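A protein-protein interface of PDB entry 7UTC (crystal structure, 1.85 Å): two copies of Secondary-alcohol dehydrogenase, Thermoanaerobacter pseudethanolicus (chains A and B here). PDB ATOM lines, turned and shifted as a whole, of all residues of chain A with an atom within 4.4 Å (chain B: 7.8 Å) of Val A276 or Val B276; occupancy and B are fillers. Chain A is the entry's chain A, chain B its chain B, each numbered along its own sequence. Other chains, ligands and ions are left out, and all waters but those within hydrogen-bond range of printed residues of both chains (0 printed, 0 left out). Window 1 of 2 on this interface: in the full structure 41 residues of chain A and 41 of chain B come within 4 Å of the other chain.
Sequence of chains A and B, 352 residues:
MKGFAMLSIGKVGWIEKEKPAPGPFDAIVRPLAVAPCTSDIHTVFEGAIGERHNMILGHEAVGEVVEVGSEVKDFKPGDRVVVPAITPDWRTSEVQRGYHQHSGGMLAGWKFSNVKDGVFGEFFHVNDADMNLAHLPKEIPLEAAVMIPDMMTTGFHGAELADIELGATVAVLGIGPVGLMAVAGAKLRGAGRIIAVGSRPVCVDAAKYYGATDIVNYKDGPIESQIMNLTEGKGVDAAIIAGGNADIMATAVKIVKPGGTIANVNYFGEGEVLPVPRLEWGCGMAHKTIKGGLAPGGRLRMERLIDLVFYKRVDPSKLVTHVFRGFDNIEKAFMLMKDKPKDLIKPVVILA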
ATOM      1  N   MET A 249      22.813 -30.422   0.845  1.00  0.00           N
ATOM      2  CA  MET A 249      22.140 -30.348  -0.445  1.00  0.00           C
ATOM      3  C   MET A 249      22.991 -29.594  -1.457  1.00  0.00           C
ATOM      4  O   MET A 249      23.102 -30.004  -2.618  1.00  0.00           O
ATOM      5  CB  MET A 249      20.774 -29.683  -0.283  1.00  0.00           C
ATOM      6  CG  MET A 249      20.022 -29.501  -1.590  1.00  0.00           C
ATOM      7  SD  MET A 249      19.739 -31.060  -2.455  1.00  0.00           S
ATOM      8  CE  MET A 249      18.535 -31.838  -1.375  1.00  0.00           C
ATOM      9  N   GLU A 272      14.832 -23.617   7.444  1.00  0.00           N
ATOM     10  CA  GLU A 272      13.621 -23.337   6.686  1.00  0.00           C
ATOM     11  C   GLU A 272      13.763 -23.687   5.213  1.00  0.00           C
ATOM     12  O   GLU A 272      12.785 -24.108   4.583  1.00  0.00           O
ATOM     13  CB  GLU A 272      13.248 -21.859   6.833  1.00  0.00           C
ATOM     14  CG  GLU A 272      11.914 -21.489   6.220  1.00  0.00           C
ATOM     15  CD  GLU A 272      11.597 -20.019   6.378  1.00  0.00           C
ATOM     16  OE1 GLU A 272      12.546 -19.212   6.462  1.00  0.00           O
ATOM     17  OE2 GLU A 272      10.397 -19.672   6.425  1.00  0.00           O
ATOM     18  N   VAL A 273      14.965 -23.546   4.662  1.00  0.00           N
ATOM     19  CA  VAL A 273      15.210 -23.669   3.234  1.00  0.00           C
ATOM     20  C   VAL A 273      16.370 -24.630   3.019  1.00  0.00           C
ATOM     21  O   VAL A 273      17.375 -24.566   3.735  1.00  0.00           O
ATOM     22  CB  VAL A 273      15.514 -22.296   2.606  1.00  0.00           C
ATOM     23  CG1 VAL A 273      16.304 -22.451   1.319  1.00  0.00           C
ATOM     24  CG2 VAL A 273      14.223 -21.528   2.368  1.00  0.00           C
ATOM     25  N   LEU A 274      16.229 -25.527   2.046  1.00  0.00           N
ATOM     26  CA  LEU A 274      17.339 -26.374   1.636  1.00  0.00           C
ATOM     27  C   LEU A 274      18.031 -25.729   0.443  1.00  0.00           C
ATOM     28  O   LEU A 274      17.402 -25.572  -0.611  1.00  0.00           O
ATOM     29  CB  LEU A 274      16.852 -27.764   1.278  1.00  0.00           C
ATOM     30  CG  LEU A 274      15.954 -28.455   2.305  1.00  0.00           C
ATOM     31  CD1 LEU A 274      15.635 -29.856   1.830  1.00  0.00           C
ATOM     32  CD2 LEU A 274      16.585 -28.488   3.694  1.00  0.00           C
ATOM     33  N   PRO A 275      19.298 -25.335   0.558  1.00  0.00           N
ATOM     34  CA  PRO A 275      19.926 -24.524  -0.495  1.00  0.00           C
ATOM     35  C   PRO A 275      20.271 -25.345  -1.731  1.00  0.00           C
ATOM     36  O   PRO A 275      20.853 -26.428  -1.633  1.00  0.00           O
ATOM     37  CB  PRO A 275      21.189 -23.982   0.184  1.00  0.00           C
ATOM     38  CG  PRO A 275      21.517 -25.012   1.215  1.00  0.00           C
ATOM     39  CD  PRO A 275      20.190 -25.530   1.715  1.00  0.00           C
ATOM     40  N   VAL A 276      19.920 -24.812  -2.896  1.00  0.00           N
ATOM     41  CA  VAL A 276      20.324 -25.362  -4.181  1.00  0.00           C
ATOM     42  C   VAL A 276      21.235 -24.342  -4.857  1.00  0.00           C
ATOM     43  O   VAL A 276      20.794 -23.230  -5.169  1.00  0.00           O
ATOM     44  CB  VAL A 276      19.119 -25.700  -5.075  1.00  0.00           C
ATOM     45  CG1 VAL A 276      19.590 -26.167  -6.445  1.00  0.00           C
ATOM     46  CG2 VAL A 276      18.262 -26.760  -4.413  1.00  0.00           C
ATOM     47  N   PRO A 277      22.508 -24.664  -5.098  1.00  0.00           N
ATOM     48  CA  PRO A 277      23.440 -23.688  -5.692  1.00  0.00           C
ATOM     49  C   PRO A 277      23.018 -23.327  -7.109  1.00  0.00           C
ATOM     50  O   PRO A 277      22.964 -24.191  -7.985  1.00  0.00           O
ATOM     51  CB  PRO A 277      24.784 -24.429  -5.683  1.00  0.00           C
ATOM     52  CG  PRO A 277      24.593 -25.613  -4.796  1.00  0.00           C
ATOM     53  CD  PRO A 277      23.148 -25.965  -4.851  1.00  0.00           C
ATOM     54  N   ARG A 278      22.730 -22.044  -7.336  1.00  0.00           N
ATOM     55  CA  ARG A 278      22.278 -21.616  -8.659  1.00  0.00           C
ATOM     56  C   ARG A 278      23.306 -21.960  -9.735  1.00  0.00           C
ATOM     57  O   ARG A 278      22.970 -22.562 -10.763  1.00  0.00           O
ATOM     58  CB  ARG A 278      21.978 -20.115  -8.662  1.00  0.00           C
ATOM     59  CG  ARG A 278      21.526 -19.591 -10.023  1.00  0.00           C
ATOM     60  CD  ARG A 278      21.371 -18.074 -10.052  1.00  0.00           C
ATOM     61  NE  ARG A 278      22.634 -17.389  -9.806  1.00  0.00           N
ATOM     62  CZ  ARG A 278      23.475 -16.995 -10.755  1.00  0.00           C
ATOM     63  NH1 ARG A 278      23.211 -17.190 -12.038  1.00  0.00           N
ATOM     64  NH2 ARG A 278      24.607 -16.387 -10.408  1.00  0.00           N
ATOM     65  N   TRP A 281      23.969 -25.691 -10.300  1.00  0.00           N
ATOM     66  CA  TRP A 281      22.795 -26.327 -10.878  1.00  0.00           C
ATOM     67  C   TRP A 281      22.544 -25.863 -12.308  1.00  0.00           C
ATOM     68  O   TRP A 281      21.458 -26.102 -12.850  1.00  0.00           O
ATOM     69  CB  TRP A 281      21.559 -26.075 -10.001  1.00  0.00           C
ATOM     70  CG  TRP A 281      20.456 -27.120 -10.132  1.00  0.00           C
ATOM     71  CD1 TRP A 281      20.596 -28.481 -10.042  1.00  0.00           C
ATOM     72  CD2 TRP A 281      19.057 -26.881 -10.355  1.00  0.00           C
ATOM     73  NE1 TRP A 281      19.376 -29.098 -10.209  1.00  0.00           N
ATOM     74  CE2 TRP A 281      18.416 -28.138 -10.401  1.00  0.00           C
ATOM     75  CE3 TRP A 281      18.285 -25.727 -10.527  1.00  0.00           C
ATOM     76  CZ2 TRP A 281      17.044 -28.273 -10.609  1.00  0.00           C
ATOM     77  CZ3 TRP A 281      16.922 -25.863 -10.735  1.00  0.00           C
ATOM     78  CH2 TRP A 281      16.316 -27.126 -10.775  1.00  0.00           C
ATOM     79  N   ILE A 290      16.873 -33.689  -8.809  1.00  0.00           N
ATOM     80  CA  ILE A 290      16.904 -33.820  -7.356  1.00  0.00           C
ATOM     81  C   ILE A 290      15.686 -34.614  -6.906  1.00  0.00           C
ATOM     82  O   ILE A 290      14.544 -34.246  -7.211  1.00  0.00           O
ATOM     83  CB  ILE A 290      16.942 -32.452  -6.666  1.00  0.00           C
ATOM     84  CG1 ILE A 290      18.112 -31.632  -7.197  1.00  0.00           C
ATOM     85  CG2 ILE A 290      17.062 -32.634  -5.164  1.00  0.00           C
ATOM     86  CD1 ILE A 290      18.054 -30.191  -6.768  1.00  0.00           C
ATOM     87  N   ALA B 246      14.330 -16.345  -7.908  1.00  0.00           N
ATOM     88  CA  ALA B 246      14.682 -17.607  -7.261  1.00  0.00           C
ATOM     89  C   ALA B 246      13.613 -18.080  -6.287  1.00  0.00           C
ATOM     90  O   ALA B 246      13.559 -19.274  -5.975  1.00  0.00           O
ATOM     91  CB  ALA B 246      16.020 -17.478  -6.530  1.00  0.00           C
ATOM     92  N   MET B 249      10.945 -21.024  -7.186  1.00  0.00           N
ATOM     93  CA  MET B 249      11.219 -22.422  -6.868  1.00  0.00           C
ATOM     94  C   MET B 249      10.500 -22.855  -5.595  1.00  0.00           C
ATOM     95  O   MET B 249       9.953 -23.962  -5.527  1.00  0.00           O
ATOM     96  CB  MET B 249      12.728 -22.632  -6.725  1.00  0.00           C
ATOM     97  CG  MET B 249      13.124 -24.049  -6.340  1.00  0.00           C
ATOM     98  SD  MET B 249      12.692 -25.250  -7.619  1.00  0.00           S
ATOM     99  CE  MET B 249      13.773 -24.726  -8.952  1.00  0.00           C
ATOM    100  N   ALA B 250      10.499 -22.001  -4.569  1.00  0.00           N
ATOM    101  CA  ALA B 250       9.757 -22.322  -3.356  1.00  0.00           C
ATOM    102  C   ALA B 250       8.263 -22.388  -3.637  1.00  0.00           C
ATOM    103  O   ALA B 250       7.557 -23.242  -3.089  1.00  0.00           O
ATOM    104  CB  ALA B 250      10.054 -21.289  -2.271  1.00  0.00           C
ATOM    105  N   THR B 251       7.769 -21.495  -4.494  1.00  0.00           N
ATOM    106  CA  THR B 251       6.354 -21.493  -4.843  1.00  0.00           C
ATOM    107  C   THR B 251       5.948 -22.799  -5.509  1.00  0.00           C
ATOM    108  O   THR B 251       4.870 -23.337  -5.233  1.00  0.00           O
ATOM    109  CB  THR B 251       6.054 -20.312  -5.761  1.00  0.00           C
ATOM    110  OG1 THR B 251       6.381 -19.095  -5.080  1.00  0.00           O
ATOM    111  CG2 THR B 251       4.586 -20.297  -6.162  1.00  0.00           C
ATOM    112  N   VAL B 253       7.291 -25.861  -5.236  1.00  0.00           N
ATOM    113  CA  VAL B 253       7.254 -26.994  -4.314  1.00  0.00           C
ATOM    114  C   VAL B 253       6.022 -26.921  -3.425  1.00  0.00           C
ATOM    115  O   VAL B 253       5.424 -27.950  -3.088  1.00  0.00           O
ATOM    116  CB  VAL B 253       8.546 -27.047  -3.478  1.00  0.00           C
ATOM    117  CG1 VAL B 253       8.456 -28.131  -2.421  1.00  0.00           C
ATOM    118  CG2 VAL B 253       9.747 -27.280  -4.371  1.00  0.00           C
ATOM    119  N   LYS B 254       5.610 -25.710  -3.044  1.00  0.00           N
ATOM    120  CA  LYS B 254       4.454 -25.568  -2.168  1.00  0.00           C
ATOM    121  C   LYS B 254       3.153 -25.947  -2.868  1.00  0.00           C
ATOM    122  O   LYS B 254       2.227 -26.438  -2.215  1.00  0.00           O
ATOM    123  CB  LYS B 254       4.390 -24.141  -1.633  1.00  0.00           C
ATOM    124  CG  LYS B 254       5.558 -23.785  -0.728  1.00  0.00           C
ATOM    125  CD  LYS B 254       5.560 -22.308  -0.361  1.00  0.00           C
ATOM    126  CE  LYS B 254       6.735 -21.952   0.543  1.00  0.00           C
ATOM    127  NZ  LYS B 254       6.832 -20.478   0.743  1.00  0.00           N
ATOM    128  N   ILE B 262       8.448 -30.912 -10.129  1.00  0.00           N
ATOM    129  CA  ILE B 262       8.782 -29.535 -10.475  1.00  0.00           C
ATOM    130  C   ILE B 262       9.724 -29.584 -11.671  1.00  0.00           C
ATOM    131  O   ILE B 262      10.837 -30.119 -11.576  1.00  0.00           O
ATOM    132  CB  ILE B 262       9.434 -28.790  -9.297  1.00  0.00           C
ATOM    133  CG1 ILE B 262       8.432 -28.563  -8.162  1.00  0.00           C
ATOM    134  CG2 ILE B 262      10.025 -27.475  -9.768  1.00  0.00           C
ATOM    135  CD1 ILE B 262       8.466 -29.638  -7.105  1.00  0.00           C
ATOM    136  N   GLY B 271      21.201 -14.218  -7.658  1.00  0.00           N
ATOM    137  CA  GLY B 271      21.160 -14.984  -6.432  1.00  0.00           C
ATOM    138  C   GLY B 271      22.091 -16.182  -6.467  1.00  0.00           C
ATOM    139  O   GLY B 271      22.435 -16.716  -7.519  1.00  0.00           O
ATOM    140  N   GLU B 272      22.513 -16.604  -5.279  1.00  0.00           N
ATOM    141  CA  GLU B 272      23.389 -17.764  -5.189  1.00  0.00           C
ATOM    142  C   GLU B 272      22.625 -19.053  -4.957  1.00  0.00           C
ATOM    143  O   GLU B 272      23.038 -20.108  -5.448  1.00  0.00           O
ATOM    144  CB  GLU B 272      24.407 -17.581  -4.064  1.00  0.00           C
ATOM    145  CG  GLU B 272      25.358 -18.757  -3.912  1.00  0.00           C
ATOM    146  CD  GLU B 272      26.211 -18.658  -2.665  1.00  0.00           C
ATOM    147  OE1 GLU B 272      25.768 -18.011  -1.690  1.00  0.00           O
ATOM    148  OE2 GLU B 272      27.325 -19.225  -2.661  1.00  0.00           O
ATOM    149  N   VAL B 273      21.511 -18.986  -4.236  1.00  0.00           N
ATOM    150  CA  VAL B 273      20.807 -20.164  -3.751  1.00  0.00           C
ATOM    151  C   VAL B 273      19.367 -20.123  -4.245  1.00  0.00           C
ATOM    152  O   VAL B 273      18.681 -19.106  -4.096  1.00  0.00           O
ATOM    153  CB  VAL B 273      20.864 -20.241  -2.214  1.00  0.00           C
ATOM    154  CG1 VAL B 273      19.772 -21.150  -1.679  1.00  0.00           C
ATOM    155  CG2 VAL B 273      22.243 -20.714  -1.767  1.00  0.00           C
ATOM    156  N   LEU B 274      18.918 -21.227  -4.844  1.00  0.00           N
ATOM    157  CA  LEU B 274      17.507 -21.409  -5.155  1.00  0.00           C
ATOM    158  C   LEU B 274      16.854 -22.096  -3.964  1.00  0.00           C
ATOM    159  O   LEU B 274      17.212 -23.242  -3.652  1.00  0.00           O
ATOM    160  CB  LEU B 274      17.328 -22.240  -6.420  1.00  0.00           C
ATOM    161  CG  LEU B 274      18.088 -21.777  -7.671  1.00  0.00           C
ATOM    162  CD1 LEU B 274      17.681 -22.589  -8.889  1.00  0.00           C
ATOM    163  CD2 LEU B 274      17.890 -20.289  -7.926  1.00  0.00           C
ATOM    164  N   PRO B 275      15.917 -21.451  -3.271  1.00  0.00           N
ATOM    165  CA  PRO B 275      15.395 -22.026  -2.025  1.00  0.00           C
ATOM    166  C   PRO B 275      14.444 -23.186  -2.275  1.00  0.00           C
ATOM    167  O   PRO B 275      13.593 -23.138  -3.165  1.00  0.00           O
ATOM    168  CB  PRO B 275      14.666 -20.844  -1.377  1.00  0.00           C
ATOM    169  CG  PRO B 275      14.219 -20.021  -2.539  1.00  0.00           C
ATOM    170  CD  PRO B 275      15.330 -20.130  -3.557  1.00  0.00           C
ATOM    171  N   VAL B 276      14.597 -24.235  -1.470  1.00  0.00           N
ATOM    172  CA  VAL B 276      13.672 -25.369  -1.467  1.00  0.00           C
ATOM    173  C   VAL B 276      13.081 -25.499  -0.069  1.00  0.00           C
ATOM    174  O   VAL B 276      13.809 -25.835   0.877  1.00  0.00           O
ATOM    175  CB  VAL B 276      14.372 -26.669  -1.894  1.00  0.00           C
ATOM    176  CG1 VAL B 276      13.475 -27.867  -1.608  1.00  0.00           C
ATOM    177  CG2 VAL B 276      14.745 -26.607  -3.370  1.00  0.00           C
ATOM    178  N   PRO B 277      11.780 -25.258   0.115  1.00  0.00           N
ATOM    179  CA  PRO B 277      11.228 -25.170   1.476  1.00  0.00           C
ATOM    180  C   PRO B 277      11.253 -26.536   2.145  1.00  0.00           C
ATOM    181  O   PRO B 277      10.702 -27.502   1.616  1.00  0.00           O
ATOM    182  CB  PRO B 277       9.794 -24.670   1.253  1.00  0.00           C
ATOM    183  CG  PRO B 277       9.714 -24.287  -0.216  1.00  0.00           C
ATOM    184  CD  PRO B 277      10.727 -25.140  -0.908  1.00  0.00           C
ATOM    185  N   ARG B 278      11.902 -26.607   3.311  1.00  0.00           N
ATOM    186  CA  ARG B 278      12.092 -27.885   3.992  1.00  0.00           C
ATOM    187  C   ARG B 278      10.763 -28.568   4.278  1.00  0.00           C
ATOM    188  O   ARG B 278      10.587 -29.757   3.987  1.00  0.00           O
ATOM    189  CB  ARG B 278      12.867 -27.678   5.294  1.00  0.00           C
ATOM    190  CG  ARG B 278      13.026 -28.957   6.104  1.00  0.00           C
ATOM    191  CD  ARG B 278      13.742 -28.707   7.422  1.00  0.00           C
ATOM    192  NE  ARG B 278      12.933 -27.924   8.348  1.00  0.00           N
ATOM    193  CZ  ARG B 278      12.170 -28.445   9.301  1.00  0.00           C
ATOM    194  NH1 ARG B 278      12.104 -29.753   9.497  1.00  0.00           N
ATOM    195  NH2 ARG B 278      11.454 -27.633  10.074  1.00  0.00           N
ATOM    196  N   LEU B 279       9.813 -27.830   4.853  1.00  0.00           N
ATOM    197  CA  LEU B 279       8.562 -28.441   5.288  1.00  0.00           C
ATOM    198  C   LEU B 279       7.719 -28.882   4.097  1.00  0.00           C
ATOM    199  O   LEU B 279       7.253 -30.027   4.046  1.00  0.00           O
ATOM    200  CB  LEU B 279       7.789 -27.469   6.177  1.00  0.00           C
ATOM    201  CG  LEU B 279       8.438 -27.146   7.525  1.00  0.00           C
ATOM    202  CD1 LEU B 279       9.400 -25.959   7.420  1.00  0.00           C
ATOM    203  CD2 LEU B 279       7.375 -26.900   8.582  1.00  0.00           C
ATOM    204  N   GLU B 280       7.519 -27.990   3.122  1.00  0.00           N
ATOM    205  CA  GLU B 280       6.701 -28.329   1.964  1.00  0.00           C
ATOM    206  C   GLU B 280       7.383 -29.320   1.031  1.00  0.00           C
ATOM    207  O   GLU B 280       6.719 -29.849   0.131  1.00  0.00           O
ATOM    208  CB  GLU B 280       6.321 -27.065   1.191  1.00  0.00           C
ATOM    209  CG  GLU B 280       5.323 -26.164   1.906  1.00  0.00           C
ATOM    210  CD  GLU B 280       5.988 -25.154   2.822  1.00  0.00           C
ATOM    211  OE1 GLU B 280       7.187 -25.315   3.120  1.00  0.00           O
ATOM    212  OE2 GLU B 280       5.314 -24.191   3.244  1.00  0.00           O
ATOM    213  N   TRP B 281       8.678 -29.583   1.212  1.00  0.00           N
ATOM    214  CA  TRP B 281       9.344 -30.682   0.528  1.00  0.00           C
ATOM    215  C   TRP B 281       9.390 -31.946   1.386  1.00  0.00           C
ATOM    216  O   TRP B 281      10.272 -32.789   1.190  1.00  0.00           O
ATOM    217  CB  TRP B 281      10.756 -30.265   0.096  1.00  0.00           C
ATOM    218  CG  TRP B 281      11.312 -31.057  -1.075  1.00  0.00           C
ATOM    219  CD1 TRP B 281      10.742 -31.209  -2.307  1.00  0.00           C
ATOM    220  CD2 TRP B 281      12.551 -31.785  -1.120  1.00  0.00           C
ATOM    221  NE1 TRP B 281      11.540 -31.986  -3.109  1.00  0.00           N
ATOM    222  CE2 TRP B 281      12.656 -32.352  -2.403  1.00  0.00           C
ATOM    223  CE3 TRP B 281      13.580 -32.010  -0.199  1.00  0.00           C
ATOM    224  CZ2 TRP B 281      13.744 -33.135  -2.785  1.00  0.00           C
ATOM    225  CZ3 TRP B 281      14.653 -32.789  -0.579  1.00  0.00           C
ATOM    226  CH2 TRP B 281      14.728 -33.342  -1.859  1.00  0.00           C
ATOM    227  N   GLY B 282       8.461 -32.086   2.331  1.00  0.00           N
ATOM    228  CA  GLY B 282       8.399 -33.270   3.173  1.00  0.00           C
ATOM    229  C   GLY B 282       9.628 -33.504   4.021  1.00  0.00           C
ATOM    230  O   GLY B 282       9.938 -34.657   4.342  1.00  0.00           O
ATOM    231  N   GLY B 284      12.502 -33.524   3.104  1.00  0.00           N
ATOM    232  CA  GLY B 284      13.372 -34.358   2.306  1.00  0.00           C
ATOM    233  C   GLY B 284      12.757 -35.634   1.777  1.00  0.00           C
ATOM    234  O   GLY B 284      13.468 -36.424   1.147  1.00  0.00           O
ATOM    235  N   LYS B 288       8.810 -35.152  -4.167  1.00  0.00           N
ATOM    236  CA  LYS B 288       8.605 -34.043  -5.093  1.00  0.00           C
ATOM    237  C   LYS B 288       9.889 -33.907  -5.897  1.00  0.00           C
ATOM    238  O   LYS B 288      10.835 -33.238  -5.489  1.00  0.00           O
ATOM    239  CB  LYS B 288       8.250 -32.767  -4.346  1.00  0.00           C
ATOM    240  CG  LYS B 288       6.968 -32.876  -3.550  1.00  0.00           C
ATOM    241  CD  LYS B 288       6.486 -31.531  -3.070  1.00  0.00           C
ATOM    242  CE  LYS B 288       5.268 -31.691  -2.175  1.00  0.00           C
ATOM    243  NZ  LYS B 288       4.718 -30.373  -1.724  1.00  0.00           N
ATOM    244  N   ILE B 290      12.547 -32.676  -8.491  1.00  0.00           N
ATOM    245  CA  ILE B 290      12.891 -31.367  -9.024  1.00  0.00           C
ATOM    246  C   ILE B 290      13.795 -31.574 -10.226  1.00  0.00           C
ATOM    247  O   ILE B 290      14.798 -32.292 -10.143  1.00  0.00           O
ATOM    248  CB  ILE B 290      13.571 -30.492  -7.958  1.00  0.00           C
ATOM    249  CG1 ILE B 290      12.605 -30.225  -6.804  1.00  0.00           C
ATOM    250  CG2 ILE B 290      14.056 -29.190  -8.566  1.00  0.00           C
ATOM    251  CD1 ILE B 290      13.253 -29.525  -5.642  1.00  0.00           C
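The backbone NH (N) of Ile A290 lies within hydrogen-bond range of the backbone carbonyl oxygen (O) of Ile B290, at 2.8 Å.
The backbone carbonyl oxygen (O) of Glu B272 is in hydrogen-bond range of the backbone NH (N) of Arg A278.
The backbone carbonyl oxygen (O) of Val B276 lies within hydrogen-bond range of the backbone NH (N) of Leu A274 (2.7 Å).
The backbone NH of Arg B278 sits at hydrogen-bond distance from the backbone carbonyl oxygen of Glu A272 (2.9 Å).
The backbone carbonyl oxygen (O) of Gly B271 sits close to the guanidinium group (NE) of Arg A278.
The backbone carbonyl oxygen (O) of Val A276 lies within hydrogen-bond range of the backbone NH (N) of Leu B274.
The backbone carbonyl oxygen (O) of Lys B288 is in hydrogen-bond range of the indole nitrogen (NE1) of Trp B281 (2.8 Å).
CA of Val A273 touches O of Val B276, at 3.5 Å.
Leu A274 touches Leu B274 (O to O, 3.8 Å).
Leu A274 touches Trp B281 (CD1 to CE3, 3.6 Å).
Pro A275 touches Val B273 (CA to CG1, 3.6 Å).
Glu B272 touches Val A276.
Val B273 touches Val A276.
Val B276 touches Val A276.
Pro A277 touches Glu B272.
Met B249 touches Trp A281 (CE to CZ3, 3.8 Å).
Ile B290 touches Trp A281.
Val A276 touches just these residues of chain B: Glu B272 (3.9 Å), Val B273 (3.4 Å), Leu B274 (2.8 Å) and Val B276 (3.7 Å).
Of chain A, only Val A273, Leu A274 and Val A276 come within 4 Å of Val B276.
Pro A277 touches just one residue of chain B: Glu B272.
Printed residues of chain B within 4 Å of Pro A275: Val B273.
Of the printed residues of chain B, Val A273 touches Pro B275 (3.5 Å) and Val B276 (3.5 Å).
Of the printed residues of chain A, Pro B275 touches Val A273.
Of the printed residues of chain A, Arg B278 touches Glu A272.
Leu B279 touches none of the printed residues of chain A.
Gly B284 touches none of the printed residues of chain A.
Hydrophobic or aromatic side chains of chain B within 4 Å of the printed part of chain A: Met B249, Val B273, Leu B274, Pro B275, Val B276, Trp B281 and Ile B290.
Along chain B the printed residues that touch a printed residue of chain A span positions 249 to 290.
Hydrophobic or aromatic side chains of chain A within 4 Å of the printed part of chain B: Val A273, Leu A274, Pro A275, Val A276 and Trp A281.
Glu A272 touches Pro B277, and with the chains exchanged Pro A277 touches Glu B272.
Val A273 touches Pro B275, and with the chains exchanged Pro A275 touches Val B273.
Val A273 touches Val B276, and with the chains exchanged Val A276 touches Val B273.
Trp A281 touches Ile B290, but with the chains exchanged Ile A290 does not touch Trp B281 (4.1 Å).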
